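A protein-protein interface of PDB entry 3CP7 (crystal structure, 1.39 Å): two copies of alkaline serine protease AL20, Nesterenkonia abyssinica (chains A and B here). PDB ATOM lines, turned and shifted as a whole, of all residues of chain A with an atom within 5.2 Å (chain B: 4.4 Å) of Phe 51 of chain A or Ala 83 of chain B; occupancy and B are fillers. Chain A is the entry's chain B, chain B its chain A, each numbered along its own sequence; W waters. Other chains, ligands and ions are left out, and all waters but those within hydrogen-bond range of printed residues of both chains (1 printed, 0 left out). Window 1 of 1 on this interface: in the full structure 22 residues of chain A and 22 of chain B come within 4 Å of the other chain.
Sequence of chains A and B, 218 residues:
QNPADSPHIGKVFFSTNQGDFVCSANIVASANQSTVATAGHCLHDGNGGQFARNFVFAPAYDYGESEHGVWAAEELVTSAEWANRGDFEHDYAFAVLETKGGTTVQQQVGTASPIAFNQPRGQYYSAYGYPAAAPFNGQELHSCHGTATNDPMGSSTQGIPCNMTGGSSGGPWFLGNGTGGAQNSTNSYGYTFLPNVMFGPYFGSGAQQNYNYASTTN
N of Leu 76 of chain A sits at hydrogen-bond distance from OD1 of Asn 84 of chain B.
2 positions are printed for both chains.
Phe 51 of chain A touches just these residues of chain B: His 44 and Ala 83.
Ala 83 of chain B touches just one residue of chain A: Phe 51 (3.6 Å).
Printed residues of chain B within 4 Å of Val 77 of chain A: Ala 80 (3.97 Å).
Printed residues of chain A within 4 Å of Ala 80 of chain B: Val 77.
The nearest printed residue of chain A that does not touch Ala 80 of chain B is Leu 76 of chain A (4.7 Å).
Hydrophobic or aromatic side chains of chain A within 4 Å of the printed part of chain B: Phe 51, Leu 76 and Val 77.
Along chain A the printed residues that touch a printed residue of chain B span positions 51 to 77.
Hydrophobic or aromatic side chains of chain B that line the printed part of chain A: His 44, Ala 80 and Ala 83.
Among the printed residues, 4 pairs touch across the chains.
Among the printed residues, no Asp or Glu carboxylate lies within 4 Å of a Lys or Arg side-chain nitrogen of the other chain.
The backbone NH of Gly 46 of chain B sits at hydrogen-bond distance from a ring nitrogen (ND1) of His 44 of chain B, 2.9 Å away.
The indole nitrogen of Trp 82 of chain B lies within hydrogen-bond range of the backbone carbonyl oxygen of His 44 of chain B.
OD1 of Asn 47 of chain B sits close to O of Asn 84 of chain B.
The backbone carbonyl oxygen (O) of Ala 80 of chain B lies within hydrogen-bond range of the side-chain amide nitrogen (ND2) of Asn 84 of chain B (2.8 Å).
His 44 of chain B touches Phe 51 of chain A.
Phe 51 of chain A touches Ala 83 of chain B (CE1 to CB, 3.6 Å).
Val 77 of chain A touches Ala 80 of chain B.
Water W1 lies within hydrogen-bond range of NE2 of His 44 of chain B (2.9 Å), O of Gly 49 of chain A (2.9 Å), N of Phe 51 of chain A (3.4 Å) and NE2 of His 44 of chain A (3.4 Å).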
ATOM      1  N   SER A  15     -15.767  14.634   9.109  1.00  0.00           N
ATOM      2  CA  SER A  15     -16.908  14.873   8.236  1.00  0.00           C
ATOM      3  C   SER A  15     -16.607  14.470   6.807  1.00  0.00           C
ATOM      4  O   SER A  15     -15.444  14.467   6.373  1.00  0.00           O
ATOM      5  CB  SER A  15     -17.340  16.343   8.294  1.00  0.00           C
ATOM      6  OG  SER A  15     -17.740  16.695   9.610  1.00  0.00           O
ATOM      7  N   LEU A  43     -10.439   8.018   7.395  1.00  0.00           N
ATOM      8  CA  LEU A  43      -9.883   9.283   6.902  1.00  0.00           C
ATOM      9  C   LEU A  43      -9.939   9.462   5.390  1.00  0.00           C
ATOM     10  O   LEU A  43      -9.548  10.509   4.867  1.00  0.00           O
ATOM     11  CB  LEU A  43      -8.476   9.563   7.477  1.00  0.00           C
ATOM     12  CG  LEU A  43      -7.361   8.517   7.473  1.00  0.00           C
ATOM     13  CD1 LEU A  43      -6.912   8.262   6.050  1.00  0.00           C
ATOM     14  CD2 LEU A  43      -6.201   9.021   8.307  1.00  0.00           C
ATOM     15  N   HIS A  44     -10.421   8.443   4.678  1.00  0.00           N
ATOM     16  CA  HIS A  44     -10.550   8.513   3.221  1.00  0.00           C
ATOM     17  C   HIS A  44     -11.684   7.624   2.725  1.00  0.00           C
ATOM     18  O   HIS A  44     -11.917   6.539   3.267  1.00  0.00           O
ATOM     19  CB  HIS A  44      -9.228   8.131   2.546  1.00  0.00           C
ATOM     20  CG  HIS A  44      -9.198   8.407   1.076  1.00  0.00           C
ATOM     21  ND1 HIS A  44      -9.740   7.543   0.150  1.00  0.00           N
ATOM     22  CD2 HIS A  44      -8.710   9.456   0.372  1.00  0.00           C
ATOM     23  CE1 HIS A  44      -9.573   8.039  -1.064  1.00  0.00           C
ATOM     24  NE2 HIS A  44      -8.955   9.201  -0.955  1.00  0.00           N
ATOM     25  N   GLY A  49     -11.432   8.748  -4.007  1.00  0.00           N
ATOM     26  CA  GLY A  49     -12.175   9.911  -3.563  1.00  0.00           C
ATOM     27  C   GLY A  49     -11.399  10.938  -2.774  1.00  0.00           C
ATOM     28  O   GLY A  49     -10.169  11.052  -2.887  1.00  0.00           O
ATOM     29  N   GLN A  50     -12.127  11.700  -1.968  1.00  0.00           N
ATOM     30  CA  GLN A  50     -11.508  12.724  -1.161  1.00  0.00           C
ATOM     31  C   GLN A  50     -11.234  12.240   0.255  1.00  0.00           C
ATOM     32  O   GLN A  50     -11.787  11.232   0.726  1.00  0.00           O
ATOM     33  CB  GLN A  50     -12.308  14.031  -1.180  1.00  0.00           C
ATOM     34  CG  GLN A  50     -13.789  13.897  -0.906  1.00  0.00           C
ATOM     35  CD  GLN A  50     -14.581  15.110  -1.372  1.00  0.00           C
ATOM     36  OE1 GLN A  50     -15.705  14.975  -1.851  1.00  0.00           O
ATOM     37  NE2 GLN A  50     -13.998  16.301  -1.239  1.00  0.00           N
ATOM     38  N   PHE A  51     -10.335  12.958   0.908  1.00  0.00           N
ATOM     39  CA  PHE A  51     -10.055  12.748   2.303  1.00  0.00           C
ATOM     40  C   PHE A  51     -11.211  13.261   3.144  1.00  0.00           C
ATOM     41  O   PHE A  51     -11.979  14.141   2.727  1.00  0.00           O
ATOM     42  CB  PHE A  51      -8.761  13.465   2.694  1.00  0.00           C
ATOM     43  CG  PHE A  51      -7.522  12.815   2.150  1.00  0.00           C
ATOM     44  CD1 PHE A  51      -6.919  13.293   0.992  1.00  0.00           C
ATOM     45  CD2 PHE A  51      -6.955  11.730   2.795  1.00  0.00           C
ATOM     46  CE1 PHE A  51      -5.774  12.686   0.480  1.00  0.00           C
ATOM     47  CE2 PHE A  51      -5.807  11.117   2.289  1.00  0.00           C
ATOM     48  CZ  PHE A  51      -5.221  11.599   1.128  1.00  0.00           C
ATOM     49  N   ALA A  52     -11.338  12.687   4.333  1.00  0.00           N
ATOM     50  CA  ALA A  52     -12.236  13.215   5.341  1.00  0.00           C
ATOM     51  C   ALA A  52     -11.853  14.654   5.661  1.00  0.00           C
ATOM     52  O   ALA A  52     -10.685  15.055   5.508  1.00  0.00           O
ATOM     53  CB  ALA A  52     -12.155  12.368   6.603  1.00  0.00           C
ATOM     54  N   ARG A  53     -12.835  15.423   6.114  1.00  0.00           N
ATOM     55  CA  ARG A  53     -12.603  16.810   6.522  1.00  0.00           C
ATOM     56  C   ARG A  53     -12.776  16.974   8.017  1.00  0.00           C
ATOM     57  O   ARG A  53     -13.478  16.193   8.661  1.00  0.00           O
ATOM     58  CB  ARG A  53     -13.543  17.760   5.775  1.00  0.00           C
ATOM     59  CG  ARG A  53     -13.290  17.800   4.274  1.00  0.00           C
ATOM     60  CD  ARG A  53     -14.145  18.834   3.570  1.00  0.00           C
ATOM     61  NE  ARG A  53     -15.573  18.542   3.672  1.00  0.00           N
ATOM     62  CZ  ARG A  53     -16.227  17.677   2.900  1.00  0.00           C
ATOM     63  NH1 ARG A  53     -17.529  17.493   3.078  1.00  0.00           N
ATOM     64  NH2 ARG A  53     -15.591  16.986   1.960  1.00  0.00           N
ATOM     65  N   LEU A  76      -3.348  13.655   6.455  1.00  0.00           N
ATOM     66  CA  LEU A  76      -3.998  12.350   6.489  1.00  0.00           C
ATOM     67  C   LEU A  76      -3.222  11.428   5.552  1.00  0.00           C
ATOM     68  O   LEU A  76      -3.018  11.773   4.375  1.00  0.00           O
ATOM     69  CB  LEU A  76      -5.465  12.490   6.069  1.00  0.00           C
ATOM     70  CG  LEU A  76      -6.258  13.464   6.951  1.00  0.00           C
ATOM     71  CD1 LEU A  76      -7.669  13.634   6.407  1.00  0.00           C
ATOM     72  CD2 LEU A  76      -6.308  12.985   8.396  1.00  0.00           C
ATOM     73  N   VAL A  77      -2.759  10.295   6.082  1.00  0.00           N
ATOM     74  CA  VAL A  77      -1.876   9.381   5.347  1.00  0.00           C
ATOM     75  C   VAL A  77      -2.514   8.000   5.258  1.00  0.00           C
ATOM     76  O   VAL A  77      -2.439   7.197   6.176  1.00  0.00           O
ATOM     77  CB  VAL A  77      -0.463   9.279   5.976  1.00  0.00           C
ATOM     78  CG1 VAL A  77       0.479   8.453   5.073  1.00  0.00           C
ATOM     79  CG2 VAL A  77       0.117  10.675   6.235  1.00  0.00           C
ATOM     80  N   THR A  78      -3.167   7.770   4.133  1.00  0.00           N
ATOM     81  CA  THR A  78      -3.891   6.555   3.842  1.00  0.00           C
ATOM     82  C   THR A  78      -3.004   5.535   3.121  1.00  0.00           C
ATOM     83  O   THR A  78      -2.114   5.916   2.364  1.00  0.00           O
ATOM     84  CB  THR A  78      -5.044   6.918   2.891  1.00  0.00           C
ATOM     85  OG1 THR A  78      -5.832   7.966   3.458  1.00  0.00           O
ATOM     86  CG2 THR A  78      -5.899   5.739   2.619  1.00  0.00           C
ATOM     87  N   HIS B  44      -3.276  13.872  -8.313  1.00  0.00           N
ATOM     88  CA  HIS B  44      -4.145  14.283  -7.215  1.00  0.00           C
ATOM     89  C   HIS B  44      -4.358  15.790  -7.249  1.00  0.00           C
ATOM     90  O   HIS B  44      -3.415  16.544  -7.503  1.00  0.00           O
ATOM     91  CB  HIS B  44      -3.573  13.840  -5.862  1.00  0.00           C
ATOM     92  CG  HIS B  44      -4.535  13.996  -4.727  1.00  0.00           C
ATOM     93  ND1 HIS B  44      -4.802  15.215  -4.146  1.00  0.00           N
ATOM     94  CD2 HIS B  44      -5.320  13.094  -4.093  1.00  0.00           C
ATOM     95  CE1 HIS B  44      -5.698  15.056  -3.186  1.00  0.00           C
ATOM     96  NE2 HIS B  44      -6.038  13.778  -3.140  1.00  0.00           N
ATOM     97  N   GLY B  46      -4.770  18.006  -4.969  1.00  0.00           N
ATOM     98  CA  GLY B  46      -4.251  18.833  -3.884  1.00  0.00           C
ATOM     99  C   GLY B  46      -5.352  19.180  -2.897  1.00  0.00           C
ATOM    100  O   GLY B  46      -6.380  18.496  -2.841  1.00  0.00           O
ATOM    101  N   ASN B  47      -5.148  20.254  -2.139  1.00  0.00           N
ATOM    102  CA  ASN B  47      -5.997  20.554  -0.974  1.00  0.00           C
ATOM    103  C   ASN B  47      -7.509  20.456  -1.232  1.00  0.00           C
ATOM    104  O   ASN B  47      -8.054  21.179  -2.071  1.00  0.00           O
ATOM    105  CB  ASN B  47      -5.630  21.912  -0.355  1.00  0.00           C
ATOM    106  CG  ASN B  47      -6.145  22.064   1.076  1.00  0.00           C
ATOM    107  OD1 ASN B  47      -6.889  21.218   1.579  1.00  0.00           O
ATOM    108  ND2 ASN B  47      -5.743  23.145   1.738  1.00  0.00           N
ATOM    109  N   THR B  78       0.387   9.541  -3.803  1.00  0.00           N
ATOM    110  CA  THR B  78       0.699  10.952  -3.660  1.00  0.00           C
ATOM    111  C   THR B  78       1.475  11.230  -2.368  1.00  0.00           C
ATOM    112  O   THR B  78       1.311  10.516  -1.382  1.00  0.00           O
ATOM    113  CB  THR B  78      -0.615  11.779  -3.689  1.00  0.00           C
ATOM    114  OG1 THR B  78      -0.310  13.163  -3.532  1.00  0.00           O
ATOM    115  CG2 THR B  78      -1.601  11.344  -2.592  1.00  0.00           C
ATOM    116  N   SER B  79       2.318  12.264  -2.367  1.00  0.00           N
ATOM    117  CA  SER B  79       2.899  12.721  -1.116  1.00  0.00           C
ATOM    118  C   SER B  79       1.775  13.227  -0.214  1.00  0.00           C
ATOM    119  O   SER B  79       0.730  13.686  -0.708  1.00  0.00           O
ATOM    120  CB  SER B  79       3.911  13.835  -1.354  1.00  0.00           C
ATOM    121  OG  SER B  79       3.235  15.045  -1.622  1.00  0.00           O
ATOM    122  N   ALA B  80       1.980  13.130   1.100  1.00  0.00           N
ATOM    123  CA  ALA B  80       0.985  13.594   2.058  1.00  0.00           C
ATOM    124  C   ALA B  80       0.818  15.092   1.986  1.00  0.00           C
ATOM    125  O   ALA B  80      -0.299  15.592   2.080  1.00  0.00           O
ATOM    126  CB  ALA B  80       1.380  13.197   3.448  1.00  0.00           C
ATOM    127  N   GLU B  81       1.921  15.811   1.840  1.00  0.00           N
ATOM    128  CA  GLU B  81       1.848  17.271   1.879  1.00  0.00           C
ATOM    129  C   GLU B  81       1.183  17.823   0.623  1.00  0.00           C
ATOM    130  O   GLU B  81       0.464  18.826   0.693  1.00  0.00           O
ATOM    131  CB  GLU B  81       3.237  17.875   2.049  1.00  0.00           C
ATOM    132  CG  GLU B  81       3.976  17.420   3.309  1.00  0.00           C
ATOM    133  CD  GLU B  81       4.810  16.153   3.122  1.00  0.00           C
ATOM    134  OE1 GLU B  81       5.672  15.884   3.998  1.00  0.00           O
ATOM    135  OE2 GLU B  81       4.619  15.430   2.125  1.00  0.00           O
ATOM    136  N   TRP B  82       1.417  17.188  -0.522  1.00  0.00           N
ATOM    137  CA  TRP B  82       0.692  17.587  -1.725  1.00  0.00           C
ATOM    138  C   TRP B  82      -0.816  17.325  -1.576  1.00  0.00           C
ATOM    139  O   TRP B  82      -1.640  18.223  -1.773  1.00  0.00           O
ATOM    140  CB  TRP B  82       1.230  16.921  -3.010  1.00  0.00           C
ATOM    141  CG  TRP B  82       0.375  17.358  -4.135  1.00  0.00           C
ATOM    142  CD1 TRP B  82      -0.661  16.670  -4.717  1.00  0.00           C
ATOM    143  CD2 TRP B  82       0.373  18.658  -4.712  1.00  0.00           C
ATOM    144  NE1 TRP B  82      -1.281  17.463  -5.658  1.00  0.00           N
ATOM    145  CE2 TRP B  82      -0.673  18.694  -5.665  1.00  0.00           C
ATOM    146  CE3 TRP B  82       1.168  19.803  -4.527  1.00  0.00           C
ATOM    147  CZ2 TRP B  82      -0.941  19.834  -6.430  1.00  0.00           C
ATOM    148  CZ3 TRP B  82       0.909  20.935  -5.297  1.00  0.00           C
ATOM    149  CH2 TRP B  82      -0.142  20.939  -6.231  1.00  0.00           C
ATOM    150  N   ALA B  83      -1.175  16.091  -1.231  1.00  0.00           N
ATOM    151  CA  ALA B  83      -2.596  15.716  -1.149  1.00  0.00           C
ATOM    152  C   ALA B  83      -3.384  16.551  -0.158  1.00  0.00           C
ATOM    153  O   ALA B  83      -4.547  16.879  -0.408  1.00  0.00           O
ATOM    154  CB  ALA B  83      -2.737  14.243  -0.790  1.00  0.00           C
ATOM    155  N   ASN B  84      -2.756  16.870   0.966  1.00  0.00           N
ATOM    156  CA  ASN B  84      -3.451  17.513   2.057  1.00  0.00           C
ATOM    157  C   ASN B  84      -3.433  19.036   1.957  1.00  0.00           C
ATOM    158  O   ASN B  84      -4.359  19.693   2.431  1.00  0.00           O
ATOM    159  CB  ASN B  84      -2.908  17.028   3.411  1.00  0.00           C
ATOM    160  CG  ASN B  84      -3.365  15.602   3.761  1.00  0.00           C
ATOM    161  OD1 ASN B  84      -4.380  15.430   4.431  1.00  0.00           O
ATOM    162  ND2 ASN B  84      -2.604  14.578   3.328  1.00  0.00           N
ATOM    163  N   ARG B  85      -2.387  19.610   1.357  1.00  0.00           N
ATOM    164  CA  ARG B  85      -2.180  21.056   1.434  1.00  0.00           C
ATOM    165  C   ARG B  85      -1.736  21.713   0.106  1.00  0.00           C
ATOM    166  O   ARG B  85      -1.601  22.935   0.036  1.00  0.00           O
ATOM    167  CB  ARG B  85      -1.183  21.375   2.576  1.00  0.00           C
ATOM    168  CG  ARG B  85      -1.491  20.644   3.921  1.00  0.00           C
ATOM    169  CD  ARG B  85      -0.563  20.999   5.091  1.00  0.00           C
ATOM    170  NE  ARG B  85       0.801  20.474   4.973  1.00  0.00           N
ATOM    171  CZ  ARG B  85       1.806  21.144   4.409  1.00  0.00           C
ATOM    172  NH1 ARG B  85       3.021  20.614   4.353  1.00  0.00           N
ATOM    173  NH2 ARG B  85       1.590  22.347   3.895  1.00  0.00           N
HETATM  174  O   HOH W   1      -8.032  12.462  -1.581  1.00  0.00           O
